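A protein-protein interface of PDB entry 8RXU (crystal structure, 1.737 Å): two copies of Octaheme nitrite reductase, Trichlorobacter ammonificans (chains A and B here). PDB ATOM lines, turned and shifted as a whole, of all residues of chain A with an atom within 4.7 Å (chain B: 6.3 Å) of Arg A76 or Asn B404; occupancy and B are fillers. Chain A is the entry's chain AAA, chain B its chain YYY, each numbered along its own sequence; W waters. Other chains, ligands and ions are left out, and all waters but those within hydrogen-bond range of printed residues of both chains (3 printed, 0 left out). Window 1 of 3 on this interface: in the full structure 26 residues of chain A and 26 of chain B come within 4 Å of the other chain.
OD2 of Asp A119 is in hydrogen-bond range of OH of Tyr B405 (2.6 Å).
The backbone carbonyl oxygen of Ala A75 is in hydrogen-bond range of the side-chain amide nitrogen of Asn B404 (3.0 Å).
The side-chain amino group (NZ) of Lys B409 is in salt-bridge range of the side-chain carboxylate (OD2) of Asp A119.
N of Ala A75 is in hydrogen-bond range of OG1 of Thr B401 (2.7 Å).
O of Thr A73 is in hydrogen-bond range of ND2 of Asn B404 (2.8 Å).
ND2 of Asn B404 sits close to O of Glu B400 (3.1 Å).
OE2 of Glu B400 lies within salt-bridge range of NH1 of Arg B403, at 2.8 Å.
The side-chain carboxylate (OE2) of Glu A101 is in salt-bridge range of the guanidinium group (NE) of Arg A76.
The backbone NH (N) of Asp A119 sits at hydrogen-bond distance from the side-chain carboxylate (OE1) of Glu A101, at 2.9 Å.
The side-chain carboxylate (OD1) of Asp A119 lies within salt-bridge range of the guanidinium group (NH2) of Arg A76, 3.5 Å away.
The guanidinium group (NH2) of Arg A76 sits at hydrogen-bond distance from the backbone carbonyl oxygen (O) of Ala A117 (3.2 Å).
Among the printed residues, pairs that only touch across the chains: Thr A73 with Glu B400, Gly A74 with Phe B397, Gly A74 with Glu B400, Gly A74 with Thr B401, Gly A74 with Asn B404, Ala A75 with Phe B397, Arg A76 with Asn B404, Arg A76 with Tyr B405, Lys A77 with Asn B404, Glu A78 with Gly B408, Glu A101 with Tyr B405, Trp A132 with Thr B401, Trp A132 with Ile B402, Trp A132 with Tyr B405 and Tyr A135 with Thr B401.
Arg A76 touches just these residues of chain B: Asn B404 (3.9 Å) and Tyr B405 (3.5 Å).
Of the printed residues of chain B, Lys A77 touches Asn B404 (3.6 Å).
Of the printed residues of chain B, Asp A119 touches Tyr B405 (2.6 Å) and Lys B409 (2.6 Å).
Asn B404 touches just these residues of chain A: Thr A73 (2.8 Å), Gly A74 (3.7 Å), Ala A75 (3.0 Å), Arg A76 (3.9 Å) and Lys A77 (3.6 Å).
Asp B460 touches none of the printed residues of chain A.
Of the 13 printed residues of chain B, 8 touch a printed residue of chain A.
Hydrophobic or aromatic side chains of chain B within 4 Å of the printed part of chain A: Phe B397, Ile B402 and Tyr B405.
Hydrophobic or aromatic side chains of chain A within 4 Å of the printed part of chain B: Ala A75, Trp A132 and Tyr A135.
Among the printed residues, Asp or Glu carboxylates within 4 Å of a Lys or Arg side-chain nitrogen of the other chain: Asp A119 with Lys B409 (2.6 Å).
No position is printed for both chains.
Of the 20 pairs that touch across the chains among the printed residues, none has its exchanged pair printed and touching as well.
Water W3 lies within hydrogen-bond range of OE1 of Glu A78 and NZ of Lys B409.
Water W1 bridges O of Asn B404 (2.6 Å) and N of Glu A78 (3.3 Å).
Water W2 lies within hydrogen-bond range of OD1 of Asp A119 (3.0 Å) and OH of Tyr B405 (3.4 Å).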
ATOM      1  N   THR A  73      14.369  27.002 -25.555  1.00  0.00           N
ATOM      2  CA  THR A  73      13.639  28.191 -25.034  1.00  0.00           C
ATOM      3  C   THR A  73      12.281  27.733 -24.484  1.00  0.00           C
ATOM      4  O   THR A  73      11.470  28.572 -24.111  1.00  0.00           O
ATOM      5  CB  THR A  73      13.556  29.268 -26.126  1.00  0.00           C
ATOM      6  OG1 THR A  73      12.722  28.913 -27.239  1.00  0.00           O
ATOM      7  CG2 THR A  73      14.924  29.630 -26.673  1.00  0.00           C
ATOM      8  N   GLY A  74      12.032  26.432 -24.470  1.00  0.00           N
ATOM      9  CA  GLY A  74      10.754  25.800 -24.083  1.00  0.00           C
ATOM     10  C   GLY A  74       9.544  26.327 -24.840  1.00  0.00           C
ATOM     11  O   GLY A  74       9.639  26.961 -25.961  1.00  0.00           O
ATOM     12  N   ALA A  75       8.405  25.950 -24.317  1.00  0.00           N
ATOM     13  CA  ALA A  75       7.091  26.222 -24.895  1.00  0.00           C
ATOM     14  C   ALA A  75       6.264  26.955 -23.859  1.00  0.00           C
ATOM     15  O   ALA A  75       6.823  27.361 -22.826  1.00  0.00           O
ATOM     16  CB  ALA A  75       6.502  24.929 -25.326  1.00  0.00           C
ATOM     17  N   ARG A  76       4.963  26.933 -24.081  1.00  0.00           N
ATOM     18  CA  ARG A  76       3.909  27.559 -23.260  1.00  0.00           C
ATOM     19  C   ARG A  76       4.286  29.026 -23.035  1.00  0.00           C
ATOM     20  O   ARG A  76       4.069  29.542 -21.928  1.00  0.00           O
ATOM     21  CB  ARG A  76       3.651  26.766 -21.976  1.00  0.00           C
ATOM     22  CG  ARG A  76       2.292  27.077 -21.379  1.00  0.00           C
ATOM     23  CD  ARG A  76       1.251  25.982 -21.467  1.00  0.00           C
ATOM     24  NE  ARG A  76       0.069  26.350 -20.696  1.00  0.00           N
ATOM     25  CZ  ARG A  76      -0.817  25.473 -20.221  1.00  0.00           C
ATOM     26  NH1 ARG A  76      -0.703  24.184 -20.481  1.00  0.00           N
ATOM     27  NH2 ARG A  76      -1.851  25.900 -19.515  1.00  0.00           N
ATOM     28  N   LYS A  77       4.852  29.670 -24.080  1.00  0.00           N
ATOM     29  CA  LYS A  77       5.361  31.060 -24.071  1.00  0.00           C
ATOM     30  C   LYS A  77       4.162  32.005 -24.105  1.00  0.00           C
ATOM     31  O   LYS A  77       3.620  32.279 -25.179  1.00  0.00           O
ATOM     32  CB  LYS A  77       6.302  31.363 -25.255  1.00  0.00           C
ATOM     33  CG  LYS A  77       7.538  30.450 -25.406  1.00  0.00           C
ATOM     34  CD  LYS A  77       8.594  31.098 -26.267  1.00  0.00           C
ATOM     35  CE  LYS A  77       9.895  30.328 -26.386  1.00  0.00           C
ATOM     36  NZ  LYS A  77      10.443  30.514 -27.750  1.00  0.00           N
ATOM     37  N   GLU A  78       3.707  32.429 -22.938  1.00  0.00           N
ATOM     38  CA  GLU A  78       2.770  33.588 -22.863  1.00  0.00           C
ATOM     39  C   GLU A  78       3.257  34.764 -23.724  1.00  0.00           C
ATOM     40  O   GLU A  78       4.469  35.172 -23.650  1.00  0.00           O
ATOM     41  CB  GLU A  78       2.568  33.925 -21.389  1.00  0.00           C
ATOM     42  CG  GLU A  78       1.606  35.083 -21.171  1.00  0.00           C
ATOM     43  CD  GLU A  78       0.198  34.851 -21.689  1.00  0.00           C
ATOM     44  OE1 GLU A  78      -0.403  33.746 -21.416  1.00  0.00           O
ATOM     45  OE2 GLU A  78      -0.327  35.780 -22.387  1.00  0.00           O
ATOM     46  N   GLU A 101      -4.888  33.519 -20.612  1.00  0.00           N
ATOM     47  CA  GLU A 101      -3.732  32.807 -21.198  1.00  0.00           C
ATOM     48  C   GLU A 101      -3.852  32.724 -22.718  1.00  0.00           C
ATOM     49  O   GLU A 101      -4.911  32.356 -23.264  1.00  0.00           O
ATOM     50  CB  GLU A 101      -3.575  31.391 -20.657  1.00  0.00           C
ATOM     51  CG  GLU A 101      -2.395  30.712 -21.322  1.00  0.00           C
ATOM     52  CD  GLU A 101      -1.931  29.389 -20.748  1.00  0.00           C
ATOM     53  OE1 GLU A 101      -2.771  28.662 -20.144  1.00  0.00           O
ATOM     54  OE2 GLU A 101      -0.739  29.094 -20.952  1.00  0.00           O
ATOM     55  N   ALA A 103      -0.667  31.616 -25.514  1.00  0.00           N
ATOM     56  CA  ALA A 103       0.760  31.289 -25.695  1.00  0.00           C
ATOM     57  C   ALA A 103       1.026  31.222 -27.195  1.00  0.00           C
ATOM     58  O   ALA A 103       0.084  31.004 -27.935  1.00  0.00           O
ATOM     59  CB  ALA A 103       1.147  29.963 -25.038  1.00  0.00           C
ATOM     60  N   ALA A 117      -5.875  21.980 -22.671  1.00  0.00           N
ATOM     61  CA  ALA A 117      -5.185  22.270 -21.382  1.00  0.00           C
ATOM     62  C   ALA A 117      -4.951  23.781 -21.143  1.00  0.00           C
ATOM     63  O   ALA A 117      -4.473  24.178 -20.033  1.00  0.00           O
ATOM     64  CB  ALA A 117      -3.896  21.504 -21.356  1.00  0.00           C
ATOM     65  N   VAL A 118      -5.176  24.629 -22.153  1.00  0.00           N
ATOM     66  CA  VAL A 118      -4.910  26.075 -21.987  1.00  0.00           C
ATOM     67  C   VAL A 118      -5.929  26.591 -20.958  1.00  0.00           C
ATOM     68  O   VAL A 118      -7.092  26.062 -20.953  1.00  0.00           O
ATOM     69  CB  VAL A 118      -4.929  26.874 -23.308  1.00  0.00           C
ATOM     70  CG1 VAL A 118      -6.346  27.148 -23.789  1.00  0.00           C
ATOM     71  CG2 VAL A 118      -4.123  28.144 -23.127  1.00  0.00           C
ATOM     72  N   ASP A 119      -5.475  27.547 -20.149  1.00  0.00           N
ATOM     73  CA  ASP A 119      -6.189  28.113 -18.966  1.00  0.00           C
ATOM     74  C   ASP A 119      -7.512  28.719 -19.445  1.00  0.00           C
ATOM     75  O   ASP A 119      -8.429  28.800 -18.587  1.00  0.00           O
ATOM     76  CB  ASP A 119      -5.332  29.111 -18.174  1.00  0.00           C
ATOM     77  CG  ASP A 119      -4.183  28.519 -17.357  1.00  0.00           C
ATOM     78  OD1 ASP A 119      -4.077  27.289 -17.250  1.00  0.00           O
ATOM     79  OD2 ASP A 119      -3.408  29.300 -16.794  1.00  0.00           O
ATOM     80  N   TRP A 132       4.188  18.647 -16.030  1.00  0.00           N
ATOM     81  CA  TRP A 132       5.243  19.249 -16.916  1.00  0.00           C
ATOM     82  C   TRP A 132       6.128  18.130 -17.511  1.00  0.00           C
ATOM     83  O   TRP A 132       6.455  18.196 -18.686  1.00  0.00           O
ATOM     84  CB  TRP A 132       6.082  20.309 -16.192  1.00  0.00           C
ATOM     85  CG  TRP A 132       5.227  21.482 -15.874  1.00  0.00           C
ATOM     86  CD1 TRP A 132       4.748  21.865 -14.656  1.00  0.00           C
ATOM     87  CD2 TRP A 132       4.561  22.278 -16.861  1.00  0.00           C
ATOM     88  NE1 TRP A 132       3.953  22.980 -14.812  1.00  0.00           N
ATOM     89  CE2 TRP A 132       3.803  23.238 -16.150  1.00  0.00           C
ATOM     90  CE3 TRP A 132       4.644  22.381 -18.262  1.00  0.00           C
ATOM     91  CZ2 TRP A 132       3.072  24.234 -16.788  1.00  0.00           C
ATOM     92  CZ3 TRP A 132       3.876  23.341 -18.884  1.00  0.00           C
ATOM     93  CH2 TRP A 132       3.131  24.275 -18.156  1.00  0.00           C
ATOM     94  N   TYR A 135       4.918  17.027 -20.961  1.00  0.00           N
ATOM     95  CA  TYR A 135       4.380  18.173 -21.749  1.00  0.00           C
ATOM     96  C   TYR A 135       4.848  18.038 -23.195  1.00  0.00           C
ATOM     97  O   TYR A 135       4.112  18.520 -24.040  1.00  0.00           O
ATOM     98  CB  TYR A 135       4.680  19.556 -21.154  1.00  0.00           C
ATOM     99  CG  TYR A 135       4.018  20.723 -21.853  1.00  0.00           C
ATOM    100  CD1 TYR A 135       2.646  20.904 -21.808  1.00  0.00           C
ATOM    101  CD2 TYR A 135       4.743  21.596 -22.642  1.00  0.00           C
ATOM    102  CE1 TYR A 135       2.034  21.983 -22.428  1.00  0.00           C
ATOM    103  CE2 TYR A 135       4.154  22.698 -23.253  1.00  0.00           C
ATOM    104  CZ  TYR A 135       2.784  22.867 -23.172  1.00  0.00           C
ATOM    105  OH  TYR A 135       2.133  23.889 -23.789  1.00  0.00           O
ATOM    106  N   PHE B 397      14.403  22.486 -22.533  1.00  0.00           N
ATOM    107  CA  PHE B 397      12.982  22.645 -22.889  1.00  0.00           C
ATOM    108  C   PHE B 397      12.219  22.595 -21.573  1.00  0.00           C
ATOM    109  O   PHE B 397      11.359  23.464 -21.307  1.00  0.00           O
ATOM    110  CB  PHE B 397      12.528  21.562 -23.856  1.00  0.00           C
ATOM    111  CG  PHE B 397      11.049  21.498 -24.076  1.00  0.00           C
ATOM    112  CD1 PHE B 397      10.452  22.284 -25.051  1.00  0.00           C
ATOM    113  CD2 PHE B 397      10.242  20.711 -23.273  1.00  0.00           C
ATOM    114  CE1 PHE B 397       9.087  22.203 -25.285  1.00  0.00           C
ATOM    115  CE2 PHE B 397       8.884  20.611 -23.531  1.00  0.00           C
ATOM    116  CZ  PHE B 397       8.304  21.386 -24.519  1.00  0.00           C
ATOM    117  N   ILE B 399      13.062  23.076 -18.262  1.00  0.00           N
ATOM    118  CA  ILE B 399      13.382  24.194 -17.320  1.00  0.00           C
ATOM    119  C   ILE B 399      12.669  25.436 -17.848  1.00  0.00           C
ATOM    120  O   ILE B 399      11.935  26.079 -17.100  1.00  0.00           O
ATOM    121  CB  ILE B 399      14.879  24.464 -17.219  1.00  0.00           C
ATOM    122  CG1 ILE B 399      15.643  23.306 -16.563  1.00  0.00           C
ATOM    123  CG2 ILE B 399      15.140  25.754 -16.478  1.00  0.00           C
ATOM    124  CD1 ILE B 399      17.126  23.479 -16.659  1.00  0.00           C
ATOM    125  N   GLU B 400      12.887  25.728 -19.121  1.00  0.00           N
ATOM    126  CA  GLU B 400      12.351  26.956 -19.741  1.00  0.00           C
ATOM    127  C   GLU B 400      10.841  26.944 -19.896  1.00  0.00           C
ATOM    128  O   GLU B 400      10.264  28.041 -19.725  1.00  0.00           O
ATOM    129  CB  GLU B 400      13.044  27.171 -21.081  1.00  0.00           C
ATOM    130  CG  GLU B 400      14.474  27.598 -20.882  1.00  0.00           C
ATOM    131  CD  GLU B 400      14.777  28.839 -20.047  1.00  0.00           C
ATOM    132  OE1 GLU B 400      13.880  29.377 -19.380  1.00  0.00           O
ATOM    133  OE2 GLU B 400      15.923  29.250 -20.053  1.00  0.00           O
ATOM    134  N   THR B 401      10.218  25.805 -20.198  1.00  0.00           N
ATOM    135  CA  THR B 401       8.745  25.665 -20.376  1.00  0.00           C
ATOM    136  C   THR B 401       8.129  26.045 -19.018  1.00  0.00           C
ATOM    137  O   THR B 401       7.141  26.838 -18.983  1.00  0.00           O
ATOM    138  CB  THR B 401       8.373  24.298 -20.962  1.00  0.00           C
ATOM    139  OG1 THR B 401       8.771  24.210 -22.340  1.00  0.00           O
ATOM    140  CG2 THR B 401       6.887  24.066 -20.955  1.00  0.00           C
ATOM    141  N   ILE B 402       8.658  25.507 -17.920  1.00  0.00           N
ATOM    142  CA  ILE B 402       8.048  25.780 -16.581  1.00  0.00           C
ATOM    143  C   ILE B 402       8.207  27.265 -16.248  1.00  0.00           C
ATOM    144  O   ILE B 402       7.205  27.868 -15.762  1.00  0.00           O
ATOM    145  CB  ILE B 402       8.637  24.888 -15.479  1.00  0.00           C
ATOM    146  CG1 ILE B 402       8.034  23.485 -15.546  1.00  0.00           C
ATOM    147  CG2 ILE B 402       8.474  25.602 -14.122  1.00  0.00           C
ATOM    148  CD1 ILE B 402       9.052  22.328 -15.503  1.00  0.00           C
ATOM    149  N   ARG B 403       9.390  27.809 -16.579  1.00  0.00           N
ATOM    150  CA  ARG B 403       9.861  29.198 -16.324  1.00  0.00           C
ATOM    151  C   ARG B 403       8.894  30.083 -17.111  1.00  0.00           C
ATOM    152  O   ARG B 403       8.342  31.122 -16.565  1.00  0.00           O
ATOM    153  CB  ARG B 403      11.343  29.339 -16.720  1.00  0.00           C
ATOM    154  CG  ARG B 403      12.357  28.827 -15.699  1.00  0.00           C
ATOM    155  CD  ARG B 403      13.522  29.725 -15.414  1.00  0.00           C
ATOM    156  NE  ARG B 403      14.415  29.829 -16.553  1.00  0.00           N
ATOM    157  CZ  ARG B 403      15.595  30.376 -16.457  1.00  0.00           C
ATOM    158  NH1 ARG B 403      16.408  30.420 -17.506  1.00  0.00           N
ATOM    159  NH2 ARG B 403      15.994  30.848 -15.290  1.00  0.00           N
ATOM    160  N   ASN B 404       8.654  29.708 -18.365  1.00  0.00           N
ATOM    161  CA  ASN B 404       7.805  30.454 -19.320  1.00  0.00           C
ATOM    162  C   ASN B 404       6.391  30.580 -18.763  1.00  0.00           C
ATOM    163  O   ASN B 404       5.894  31.753 -18.715  1.00  0.00           O
ATOM    164  CB  ASN B 404       7.791  29.774 -20.682  1.00  0.00           C
ATOM    165  CG  ASN B 404       9.077  29.962 -21.475  1.00  0.00           C
ATOM    166  OD1 ASN B 404       9.896  30.883 -21.245  1.00  0.00           O
ATOM    167  ND2 ASN B 404       9.232  29.103 -22.477  1.00  0.00           N
ATOM    168  N   TYR B 405       5.831  29.468 -18.311  1.00  0.00           N
ATOM    169  CA  TYR B 405       4.422  29.405 -17.846  1.00  0.00           C
ATOM    170  C   TYR B 405       4.343  30.244 -16.559  1.00  0.00           C
ATOM    171  O   TYR B 405       3.485  31.137 -16.469  1.00  0.00           O
ATOM    172  CB  TYR B 405       3.928  27.983 -17.642  1.00  0.00           C
ATOM    173  CG  TYR B 405       2.517  27.972 -17.105  1.00  0.00           C
ATOM    174  CD1 TYR B 405       1.433  28.141 -17.952  1.00  0.00           C
ATOM    175  CD2 TYR B 405       2.284  27.948 -15.741  1.00  0.00           C
ATOM    176  CE1 TYR B 405       0.122  28.132 -17.489  1.00  0.00           C
ATOM    177  CE2 TYR B 405       0.984  27.913 -15.259  1.00  0.00           C
ATOM    178  CZ  TYR B 405      -0.091  28.039 -16.116  1.00  0.00           C
ATOM    179  OH  TYR B 405      -1.376  28.101 -15.635  1.00  0.00           O
ATOM    180  N   THR B 406       5.220  29.980 -15.596  1.00  0.00           N
ATOM    181  CA  THR B 406       5.321  30.752 -14.320  1.00  0.00           C
ATOM    182  C   THR B 406       5.504  32.257 -14.606  1.00  0.00           C
ATOM    183  O   THR B 406       4.744  33.086 -14.036  1.00  0.00           O
ATOM    184  CB  THR B 406       6.455  30.240 -13.433  1.00  0.00           C
ATOM    185  OG1 THR B 406       6.414  28.825 -13.221  1.00  0.00           O
ATOM    186  CG2 THR B 406       6.426  30.937 -12.088  1.00  0.00           C
ATOM    187  N   LYS B 407       6.436  32.606 -15.477  1.00  0.00           N
ATOM    188  CA  LYS B 407       6.796  34.053 -15.683  1.00  0.00           C
ATOM    189  C   LYS B 407       5.578  34.728 -16.321  1.00  0.00           C
ATOM    190  O   LYS B 407       5.274  35.954 -15.997  1.00  0.00           O
ATOM    191  CB  LYS B 407       8.081  34.189 -16.495  1.00  0.00           C
ATOM    192  CG  LYS B 407       9.370  33.976 -15.716  1.00  0.00           C
ATOM    193  CD  LYS B 407      10.552  34.211 -16.610  1.00  0.00           C
ATOM    194  CE  LYS B 407      10.464  33.343 -17.849  1.00  0.00           C
ATOM    195  NZ  LYS B 407      11.430  33.759 -18.895  1.00  0.00           N
ATOM    196  N   GLY B 408       4.859  34.009 -17.180  1.00  0.00           N
ATOM    197  CA  GLY B 408       3.603  34.491 -17.774  1.00  0.00           C
ATOM    198  C   GLY B 408       2.667  34.953 -16.653  1.00  0.00           C
ATOM    199  O   GLY B 408       2.139  36.060 -16.757  1.00  0.00           O
ATOM    200  N   LYS B 409       2.511  34.158 -15.599  1.00  0.00           N
ATOM    201  CA  LYS B 409       1.582  34.518 -14.478  1.00  0.00           C
ATOM    202  C   LYS B 409       2.202  35.589 -13.596  1.00  0.00           C
ATOM    203  O   LYS B 409       1.393  36.385 -13.062  1.00  0.00           O
ATOM    204  CB  LYS B 409       1.156  33.295 -13.666  1.00  0.00           C
ATOM    205  CG  LYS B 409       0.529  32.211 -14.494  1.00  0.00           C
ATOM    206  CD  LYS B 409      -0.700  32.648 -15.195  1.00  0.00           C
ATOM    207  CE  LYS B 409      -1.030  31.677 -16.288  1.00  0.00           C
ATOM    208  NZ  LYS B 409      -2.438  31.692 -16.675  1.00  0.00           N
ATOM    209  N   ASP B 460      12.024  31.153 -11.048  1.00  0.00           N
ATOM    210  CA  ASP B 460      10.843  31.414 -11.929  1.00  0.00           C
ATOM    211  C   ASP B 460       9.921  30.169 -12.030  1.00  0.00           C
ATOM    212  O   ASP B 460       9.508  29.718 -13.128  1.00  0.00           O
ATOM    213  CB  ASP B 460      11.271  32.042 -13.262  1.00  0.00           C
ATOM    214  CG  ASP B 460      11.975  33.356 -13.068  1.00  0.00           C
ATOM    215  OD1 ASP B 460      11.299  34.281 -12.518  1.00  0.00           O
ATOM    216  OD2 ASP B 460      13.225  33.435 -13.351  1.00  0.00           O
HETATM  217  O   HOH W   1       6.179  33.103 -20.863  1.00  0.00           O
HETATM  218  O   HOH W   2      -2.708  24.966 -15.991  1.00  0.00           O
HETATM  219  O   HOH W   3      -1.123  33.328 -19.164  1.00  0.00           O
